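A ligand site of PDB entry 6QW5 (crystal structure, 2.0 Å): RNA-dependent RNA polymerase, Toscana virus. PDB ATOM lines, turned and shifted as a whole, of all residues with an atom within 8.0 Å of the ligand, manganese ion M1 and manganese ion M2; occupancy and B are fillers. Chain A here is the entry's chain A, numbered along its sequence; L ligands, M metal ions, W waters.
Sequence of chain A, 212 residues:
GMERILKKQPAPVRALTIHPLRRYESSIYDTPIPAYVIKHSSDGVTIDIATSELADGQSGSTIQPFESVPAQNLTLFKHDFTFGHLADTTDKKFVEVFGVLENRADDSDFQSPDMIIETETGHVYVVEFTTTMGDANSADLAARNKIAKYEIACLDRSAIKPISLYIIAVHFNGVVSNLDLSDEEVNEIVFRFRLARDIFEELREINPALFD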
ATOM      1  N   THR A  75       5.377  10.232  20.134  1.00  0.00           N
ATOM      2  CA  THR A  75       5.438   8.993  20.913  1.00  0.00           C
ATOM      3  C   THR A  75       4.211   8.117  20.703  1.00  0.00           C
ATOM      4  O   THR A  75       4.265   6.904  20.952  1.00  0.00           O
ATOM      5  CB  THR A  75       5.580   9.309  22.407  1.00  0.00           C
ATOM      6  OG1 THR A  75       4.448  10.069  22.825  1.00  0.00           O
ATOM      7  CG2 THR A  75       6.832  10.117  22.674  1.00  0.00           C
ATOM      8  N   LEU A  76       3.095   8.697  20.257  1.00  0.00           N
ATOM      9  CA  LEU A  76       1.895   7.915  19.993  1.00  0.00           C
ATOM     10  C   LEU A  76       1.653   7.722  18.501  1.00  0.00           C
ATOM     11  O   LEU A  76       0.531   7.434  18.092  1.00  0.00           O
ATOM     12  CB  LEU A  76       0.687   8.578  20.662  1.00  0.00           C
ATOM     13  CG  LEU A  76       0.673   8.432  22.184  1.00  0.00           C
ATOM     14  CD1 LEU A  76      -0.666   8.915  22.748  1.00  0.00           C
ATOM     15  CD2 LEU A  76       0.959   6.996  22.610  1.00  0.00           C
ATOM     16  N   HIS A  79       0.051   4.280  17.373  1.00  0.00           N
ATOM     17  CA  HIS A  79      -1.354   4.295  17.772  1.00  0.00           C
ATOM     18  C   HIS A  79      -2.136   5.295  16.919  1.00  0.00           C
ATOM     19  O   HIS A  79      -3.150   4.933  16.307  1.00  0.00           O
ATOM     20  CB  HIS A  79      -1.412   4.621  19.269  1.00  0.00           C
ATOM     21  CG  HIS A  79      -2.782   4.806  19.838  1.00  0.00           C
ATOM     22  ND1 HIS A  79      -3.474   5.990  19.728  1.00  0.00           N
ATOM     23  CD2 HIS A  79      -3.544   3.985  20.594  1.00  0.00           C
ATOM     24  CE1 HIS A  79      -4.629   5.890  20.365  1.00  0.00           C
ATOM     25  NE2 HIS A  79      -4.694   4.683  20.904  1.00  0.00           N
ATOM     26  N   ASP A  80      -1.644   6.520  16.794  1.00  0.00           N
ATOM     27  CA  ASP A  80      -2.443   7.554  16.140  1.00  0.00           C
ATOM     28  C   ASP A  80      -2.460   7.440  14.620  1.00  0.00           C
ATOM     29  O   ASP A  80      -3.503   7.668  13.998  1.00  0.00           O
ATOM     30  CB  ASP A  80      -1.953   8.925  16.579  1.00  0.00           C
ATOM     31  CG  ASP A  80      -2.288   9.209  18.040  1.00  0.00           C
ATOM     32  OD1 ASP A  80      -3.433   8.893  18.476  1.00  0.00           O
ATOM     33  OD2 ASP A  80      -1.401   9.724  18.739  1.00  0.00           O
ATOM     34  N   PHE A  83      -5.157   4.685  13.528  1.00  0.00           N
ATOM     35  CA  PHE A  83      -6.570   5.059  13.601  1.00  0.00           C
ATOM     36  C   PHE A  83      -6.815   6.504  13.163  1.00  0.00           C
ATOM     37  O   PHE A  83      -7.840   7.086  13.523  1.00  0.00           O
ATOM     38  CB  PHE A  83      -7.097   4.821  15.028  1.00  0.00           C
ATOM     39  CG  PHE A  83      -6.905   3.407  15.508  1.00  0.00           C
ATOM     40  CD1 PHE A  83      -7.805   2.415  15.158  1.00  0.00           C
ATOM     41  CD2 PHE A  83      -5.797   3.063  16.270  1.00  0.00           C
ATOM     42  CE1 PHE A  83      -7.629   1.104  15.582  1.00  0.00           C
ATOM     43  CE2 PHE A  83      -5.619   1.754  16.718  1.00  0.00           C
ATOM     44  CZ  PHE A  83      -6.529   0.770  16.372  1.00  0.00           C
ATOM     45  N   THR A  89      -7.985  13.572  16.045  1.00  0.00           N
ATOM     46  CA  THR A  89      -7.124  13.499  17.213  1.00  0.00           C
ATOM     47  C   THR A  89      -7.761  12.475  18.148  1.00  0.00           C
ATOM     48  O   THR A  89      -8.873  12.007  17.916  1.00  0.00           O
ATOM     49  CB  THR A  89      -7.019  14.863  17.898  1.00  0.00           C
ATOM     50  OG1 THR A  89      -6.463  14.692  19.221  1.00  0.00           O
ATOM     51  CG2 THR A  89      -8.393  15.502  18.006  1.00  0.00           C
ATOM     52  N   THR A  90      -7.062  12.149  19.235  1.00  0.00           N
ATOM     53  CA  THR A  90      -7.652  11.303  20.261  1.00  0.00           C
ATOM     54  C   THR A  90      -7.541  11.984  21.622  1.00  0.00           C
ATOM     55  O   THR A  90      -7.016  13.106  21.748  1.00  0.00           O
ATOM     56  CB  THR A  90      -7.022   9.899  20.285  1.00  0.00           C
ATOM     57  OG1 THR A  90      -5.597   9.998  20.401  1.00  0.00           O
ATOM     58  CG2 THR A  90      -7.378   9.110  19.034  1.00  0.00           C
ATOM     59  N   ASP A  91      -8.080  11.300  22.636  1.00  0.00           N
ATOM     60  CA  ASP A  91      -8.097  11.711  24.038  1.00  0.00           C
ATOM     61  C   ASP A  91      -9.004  12.916  24.302  1.00  0.00           C
ATOM     62  O   ASP A  91      -8.658  14.057  23.983  1.00  0.00           O
ATOM     63  CB  ASP A  91      -6.676  11.969  24.516  1.00  0.00           C
ATOM     64  CG  ASP A  91      -5.806  10.717  24.471  1.00  0.00           C
ATOM     65  OD1 ASP A  91      -6.324   9.615  24.179  1.00  0.00           O
ATOM     66  OD2 ASP A  91      -4.583  10.819  24.724  1.00  0.00           O
ATOM     67  N   LYS A  92     -10.179  12.658  24.903  1.00  0.00           N
ATOM     68  CA  LYS A  92     -11.073  13.678  25.439  1.00  0.00           C
ATOM     69  C   LYS A  92     -11.396  13.309  26.879  1.00  0.00           C
ATOM     70  O   LYS A  92     -11.741  12.154  27.157  1.00  0.00           O
ATOM     71  CB  LYS A  92     -12.377  13.764  24.619  1.00  0.00           C
ATOM     72  CG  LYS A  92     -13.228  14.975  24.940  1.00  0.00           C
ATOM     73  CD  LYS A  92     -14.165  15.336  23.805  1.00  0.00           C
ATOM     74  CE  LYS A  92     -14.518  16.808  23.861  1.00  0.00           C
ATOM     75  NZ  LYS A  92     -15.352  17.250  22.696  1.00  0.00           N
ATOM     76  N   SER A 112      -9.208  10.015  29.938  1.00  0.00           N
ATOM     77  CA  SER A 112      -9.446  10.525  28.598  1.00  0.00           C
ATOM     78  C   SER A 112      -9.329   9.391  27.589  1.00  0.00           C
ATOM     79  O   SER A 112      -8.260   9.127  27.046  1.00  0.00           O
ATOM     80  CB  SER A 112      -8.470  11.660  28.243  1.00  0.00           C
ATOM     81  OG  SER A 112      -7.145  11.305  28.610  1.00  0.00           O
ATOM     82  N   PRO A 113     -10.444   8.704  27.320  1.00  0.00           N
ATOM     83  CA  PRO A 113     -10.433   7.712  26.234  1.00  0.00           C
ATOM     84  C   PRO A 113     -10.227   8.412  24.899  1.00  0.00           C
ATOM     85  O   PRO A 113     -10.272   9.636  24.797  1.00  0.00           O
ATOM     86  CB  PRO A 113     -11.803   7.025  26.334  1.00  0.00           C
ATOM     87  CG  PRO A 113     -12.640   7.905  27.230  1.00  0.00           C
ATOM     88  CD  PRO A 113     -11.732   8.786  28.022  1.00  0.00           C
ATOM     89  N   ASP A 114      -9.957   7.609  23.859  1.00  0.00           N
ATOM     90  CA  ASP A 114      -9.583   8.179  22.569  1.00  0.00           C
ATOM     91  C   ASP A 114     -10.718   8.985  21.946  1.00  0.00           C
ATOM     92  O   ASP A 114     -10.447   9.947  21.228  1.00  0.00           O
ATOM     93  CB  ASP A 114      -9.134   7.065  21.610  1.00  0.00           C
ATOM     94  CG  ASP A 114      -7.767   6.522  21.964  1.00  0.00           C
ATOM     95  OD1 ASP A 114      -6.891   7.287  22.431  1.00  0.00           O
ATOM     96  OD2 ASP A 114      -7.576   5.304  21.797  1.00  0.00           O
ATOM     97  N   MET A 115     -11.972   8.603  22.168  1.00  0.00           N
ATOM     98  CA  MET A 115     -13.108   9.404  21.678  1.00  0.00           C
ATOM     99  C   MET A 115     -14.257   9.400  22.689  1.00  0.00           C
ATOM    100  O   MET A 115     -14.539   8.386  23.318  1.00  0.00           O
ATOM    101  CB  MET A 115     -13.634   8.896  20.331  1.00  0.00           C
ATOM    102  CG  MET A 115     -12.603   8.633  19.233  1.00  0.00           C
ATOM    103  SD  MET A 115     -13.505   8.076  17.570  1.00  0.00           S
ATOM    104  CE  MET A 115     -13.895   9.865  16.828  1.00  0.00           C
ATOM    105  N   VAL A 127     -15.035   5.555  22.859  1.00  0.00           N
ATOM    106  CA  VAL A 127     -14.249   4.704  21.944  1.00  0.00           C
ATOM    107  C   VAL A 127     -12.788   4.691  22.383  1.00  0.00           C
ATOM    108  O   VAL A 127     -12.187   5.752  22.583  1.00  0.00           O
ATOM    109  CB  VAL A 127     -14.350   5.162  20.480  1.00  0.00           C
ATOM    110  CG1 VAL A 127     -13.711   4.116  19.545  1.00  0.00           C
ATOM    111  CG2 VAL A 127     -15.807   5.450  20.062  1.00  0.00           C
ATOM    112  N   GLU A 128     -12.206   3.505  22.537  1.00  0.00           N
ATOM    113  CA  GLU A 128     -10.789   3.394  22.850  1.00  0.00           C
ATOM    114  C   GLU A 128     -10.108   2.526  21.800  1.00  0.00           C
ATOM    115  O   GLU A 128     -10.633   1.468  21.447  1.00  0.00           O
ATOM    116  CB  GLU A 128     -10.542   2.834  24.242  1.00  0.00           C
ATOM    117  CG  GLU A 128      -9.045   2.689  24.611  1.00  0.00           C
ATOM    118  CD  GLU A 128      -8.282   4.010  24.682  1.00  0.00           C
ATOM    119  OE1 GLU A 128      -8.923   5.072  24.853  1.00  0.00           O
ATOM    120  OE2 GLU A 128      -7.041   3.996  24.569  1.00  0.00           O
ATOM    121  N   PHE A 129      -8.987   3.009  21.296  1.00  0.00           N
ATOM    122  CA  PHE A 129      -8.132   2.290  20.359  1.00  0.00           C
ATOM    123  C   PHE A 129      -6.902   1.754  21.073  1.00  0.00           C
ATOM    124  O   PHE A 129      -6.350   2.386  21.986  1.00  0.00           O
ATOM    125  CB  PHE A 129      -7.653   3.198  19.212  1.00  0.00           C
ATOM    126  CG  PHE A 129      -8.738   4.003  18.550  1.00  0.00           C
ATOM    127  CD1 PHE A 129      -9.849   3.379  18.018  1.00  0.00           C
ATOM    128  CD2 PHE A 129      -8.618   5.389  18.433  1.00  0.00           C
ATOM    129  CE1 PHE A 129     -10.844   4.114  17.387  1.00  0.00           C
ATOM    130  CE2 PHE A 129      -9.614   6.131  17.810  1.00  0.00           C
ATOM    131  CZ  PHE A 129     -10.721   5.496  17.287  1.00  0.00           C
ATOM    132  N   THR A 130      -6.413   0.618  20.598  1.00  0.00           N
ATOM    133  CA  THR A 130      -5.177   0.083  21.136  1.00  0.00           C
ATOM    134  C   THR A 130      -4.555  -0.814  20.072  1.00  0.00           C
ATOM    135  O   THR A 130      -5.200  -1.194  19.101  1.00  0.00           O
ATOM    136  CB  THR A 130      -5.448  -0.669  22.458  1.00  0.00           C
ATOM    137  OG1 THR A 130      -4.209  -0.987  23.110  1.00  0.00           O
ATOM    138  CG2 THR A 130      -6.245  -1.925  22.215  1.00  0.00           C
ATOM    139  N   THR A 131      -3.266  -1.082  20.237  1.00  0.00           N
ATOM    140  CA  THR A 131      -2.487  -1.899  19.308  1.00  0.00           C
ATOM    141  C   THR A 131      -1.692  -2.920  20.117  1.00  0.00           C
ATOM    142  O   THR A 131      -1.483  -2.754  21.317  1.00  0.00           O
ATOM    143  CB  THR A 131      -1.506  -1.053  18.474  1.00  0.00           C
ATOM    144  OG1 THR A 131      -0.344  -0.736  19.264  1.00  0.00           O
ATOM    145  CG2 THR A 131      -2.137   0.249  18.031  1.00  0.00           C
ATOM    146  N   ALA A 142      -5.619  -7.051  25.053  1.00  0.00           N
ATOM    147  CA  ALA A 142      -5.501  -5.602  25.091  1.00  0.00           C
ATOM    148  C   ALA A 142      -6.880  -4.922  25.077  1.00  0.00           C
ATOM    149  O   ALA A 142      -7.092  -3.934  25.783  1.00  0.00           O
ATOM    150  CB  ALA A 142      -4.646  -5.107  23.914  1.00  0.00           C
ATOM    151  N   LYS A 146      -8.496  -2.458  27.996  1.00  0.00           N
ATOM    152  CA  LYS A 146      -9.076  -1.122  27.830  1.00  0.00           C
ATOM    153  C   LYS A 146     -10.492  -1.053  28.402  1.00  0.00           C
ATOM    154  O   LYS A 146     -10.892  -0.027  28.966  1.00  0.00           O
ATOM    155  CB  LYS A 146      -9.096  -0.721  26.349  1.00  0.00           C
ATOM    156  CG  LYS A 146      -7.717  -0.503  25.741  1.00  0.00           C
ATOM    157  CD  LYS A 146      -6.872   0.408  26.626  1.00  0.00           C
ATOM    158  CE  LYS A 146      -5.595   0.842  25.898  1.00  0.00           C
ATOM    159  NZ  LYS A 146      -4.784   1.804  26.712  1.00  0.00           N
ATOM    160  N   LYS A 149     -10.059  -0.672  32.042  1.00  0.00           N
ATOM    161  CA  LYS A 149      -9.549   0.647  32.397  1.00  0.00           C
ATOM    162  C   LYS A 149     -10.648   1.706  32.454  1.00  0.00           C
ATOM    163  O   LYS A 149     -10.572   2.626  33.282  1.00  0.00           O
ATOM    164  CB  LYS A 149      -8.476   1.049  31.385  1.00  0.00           C
ATOM    165  CG  LYS A 149      -7.961   2.458  31.519  1.00  0.00           C
ATOM    166  CD  LYS A 149      -6.933   2.739  30.425  1.00  0.00           C
ATOM    167  CE  LYS A 149      -6.226   4.058  30.628  1.00  0.00           C
ATOM    168  NZ  LYS A 149      -5.320   4.010  31.811  1.00  0.00           N
ATOM    169  N   TYR A 150     -11.670   1.608  31.614  1.00  0.00           N
ATOM    170  CA  TYR A 150     -12.663   2.670  31.525  1.00  0.00           C
ATOM    171  C   TYR A 150     -14.061   2.270  32.000  1.00  0.00           C
ATOM    172  O   TYR A 150     -14.927   3.140  32.069  1.00  0.00           O
ATOM    173  CB  TYR A 150     -12.750   3.195  30.075  1.00  0.00           C
ATOM    174  CG  TYR A 150     -11.505   3.922  29.627  1.00  0.00           C
ATOM    175  CD1 TYR A 150     -11.137   5.128  30.193  1.00  0.00           C
ATOM    176  CD2 TYR A 150     -10.678   3.387  28.645  1.00  0.00           C
ATOM    177  CE1 TYR A 150      -9.982   5.803  29.791  1.00  0.00           C
ATOM    178  CE2 TYR A 150      -9.515   4.040  28.236  1.00  0.00           C
ATOM    179  CZ  TYR A 150      -9.180   5.252  28.803  1.00  0.00           C
ATOM    180  OH  TYR A 150      -8.034   5.912  28.411  1.00  0.00           O
ATOM    181  N   ILE A 168     -11.403  -0.960  19.634  1.00  0.00           N
ATOM    182  CA  ILE A 168     -10.720  -1.541  18.480  1.00  0.00           C
ATOM    183  C   ILE A 168      -9.276  -1.834  18.900  1.00  0.00           C
ATOM    184  O   ILE A 168      -8.521  -0.905  19.231  1.00  0.00           O
ATOM    185  CB  ILE A 168     -10.728  -0.614  17.249  1.00  0.00           C
ATOM    186  CG1 ILE A 168     -12.122  -0.066  16.938  1.00  0.00           C
ATOM    187  CG2 ILE A 168     -10.131  -1.342  16.038  1.00  0.00           C
ATOM    188  CD1 ILE A 168     -12.134   0.871  15.699  1.00  0.00           C
HETATM  189  O1  LIG L   1      -4.844   5.849  23.792  1.00  0.00           O
HETATM  190  C1  LIG L   1      -3.770   5.324  24.430  1.00  0.00           C
HETATM  191  C2  LIG L   1      -3.492   3.983  24.349  1.00  0.00           C
HETATM  192  O2  LIG L   1      -4.164   3.161  23.647  1.00  0.00           O
HETATM  193  O3  LIG L   1      -2.534   3.507  25.003  1.00  0.00           O
HETATM  194  C3  LIG L   1      -2.950   6.107  25.178  1.00  0.00           C
HETATM  195  C4  LIG L   1      -3.069   7.573  25.424  1.00  0.00           C
HETATM  196  C5  LIG L   1      -1.948   8.287  26.183  1.00  0.00           C
HETATM  197  C6  LIG L   1      -0.886   7.529  26.716  1.00  0.00           C
HETATM  198  C7  LIG L   1       0.158   8.136  27.426  1.00  0.00           C
HETATM  199  C8  LIG L   1       0.162   9.523  27.616  1.00  0.00           C
HETATM  200  C9  LIG L   1      -0.901  10.281  27.083  1.00  0.00           C
HETATM  201  C10 LIG L   1      -1.948   9.667  26.378  1.00  0.00           C
HETATM  202  O4  LIG L   1      -4.085   8.247  25.206  1.00  0.00           O
HETATM  203 MN    MN M   1      -5.813   4.276  22.776  1.00  0.00          MN
HETATM  204 MN    MN M   2      -5.529   7.775  23.855  1.00  0.00          MN
HETATM  205  O   HOH W   1      -2.587   1.096  23.445  1.00  0.00           O
HETATM  206  O   HOH W   2      -6.880   7.178  25.483  1.00  0.00           O
HETATM  207  O   HOH W   3      -4.433   8.563  22.325  1.00  0.00           O
HETATM  208  O   HOH W   4      -5.248  10.028  27.183  1.00  0.00           O
HETATM  209  O   HOH W   5      -1.847   1.105  25.928  1.00  0.00           O
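The side-chain amino group of Lys 146 is in salt-bridge range of an oxygen (O3) of the ligand.
O of Glu 128 sits at hydrogen-bond distance from N of Ile 168 (3.1 Å). A ring nitrogen (ND1) of His 79 sits at hydrogen-bond distance from the side-chain carboxylate (OD1) of Asp 80 (3.2 Å). O of Val 127 is in hydrogen-bond range of N of Asp 114 (3.2 Å). The backbone NH of Asp 91 sits close to the backbone carbonyl oxygen of Pro 113. The side-chain amino group (NZ) of Lys 146 lies close to the side-chain carboxylate (OE2) of Glu 128.
Residues that only touch the ligand: Leu 76. Hydrophobic or aromatic side chains within 4 Å of the ligand: Leu 76 and His 79. Of the 23 residues printed, 7 come within 4 Å of the ligand. Along chain A the residues within 4 Å of the ligand span positions 76 to 146. The nearest printed residue that does not touch the ligand is Thr 130 (4.1 Å).
Four residues have an atom within 4 Å of manganese ion M1: His 79, Asp 114, Glu 128 and Phe 129.
Of the 23 residues printed, 2 come within 4 Å of manganese ion M2. Along chain A the residues within 4 Å of manganese ion M2 span positions 91 to 114.
O1 of the ligand is bound to manganese ion M1 (2.1 Å). Manganese ion M1 is bound by O of Phe 129 (2.1 Å). Manganese ion M1 is bound by O2 of the ligand (2.2 Å). OE2 of Glu 128 is bound to manganese ion M1 (2.2 Å). A ring nitrogen (NE2) of His 79 binds manganese ion M1 (2.2 Å). OD2 of Asp 114 is bound to manganese ion M1 (2.3 Å). Manganese ion M1 has six donor atoms within binding distance.
The side-chain carboxylate (OD1) of Asp 114 binds manganese ion M2, 2.0 Å away. The side-chain carboxylate (OD1) of Asp 91 is bound to manganese ion M2 (2.0 Å). O4 of the ligand is bound to manganese ion M2, at 2.0 Å. Water W3 is bound to manganese ion M2 (2.0 Å). Manganese ion M2 is bound by an oxygen (O1) of the ligand (2.0 Å). Water W2 binds manganese ion M2. Manganese ion M2 has six donor atoms within binding distance.
Water W2 lies within hydrogen-bond range of O of Ser 112 (2.9 Å), OE1 of Glu 128 (3.0 Å) and OH of Tyr 150 (3.4 Å). Water W3 bridges OG1 of Thr 90 and OD2 of Asp 91. Water W1 bridges the side-chain hydroxyl of Thr 130 (2.7 Å) and an oxygen (O3) of the ligand (2.9 Å). Water W5 lies within hydrogen-bond range of O3 of the ligand (2.7 Å) and NZ of Lys 146 (3.1 Å). Water W4 lies within hydrogen-bond range of OD2 of Asp 91 and OG of Ser 112.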
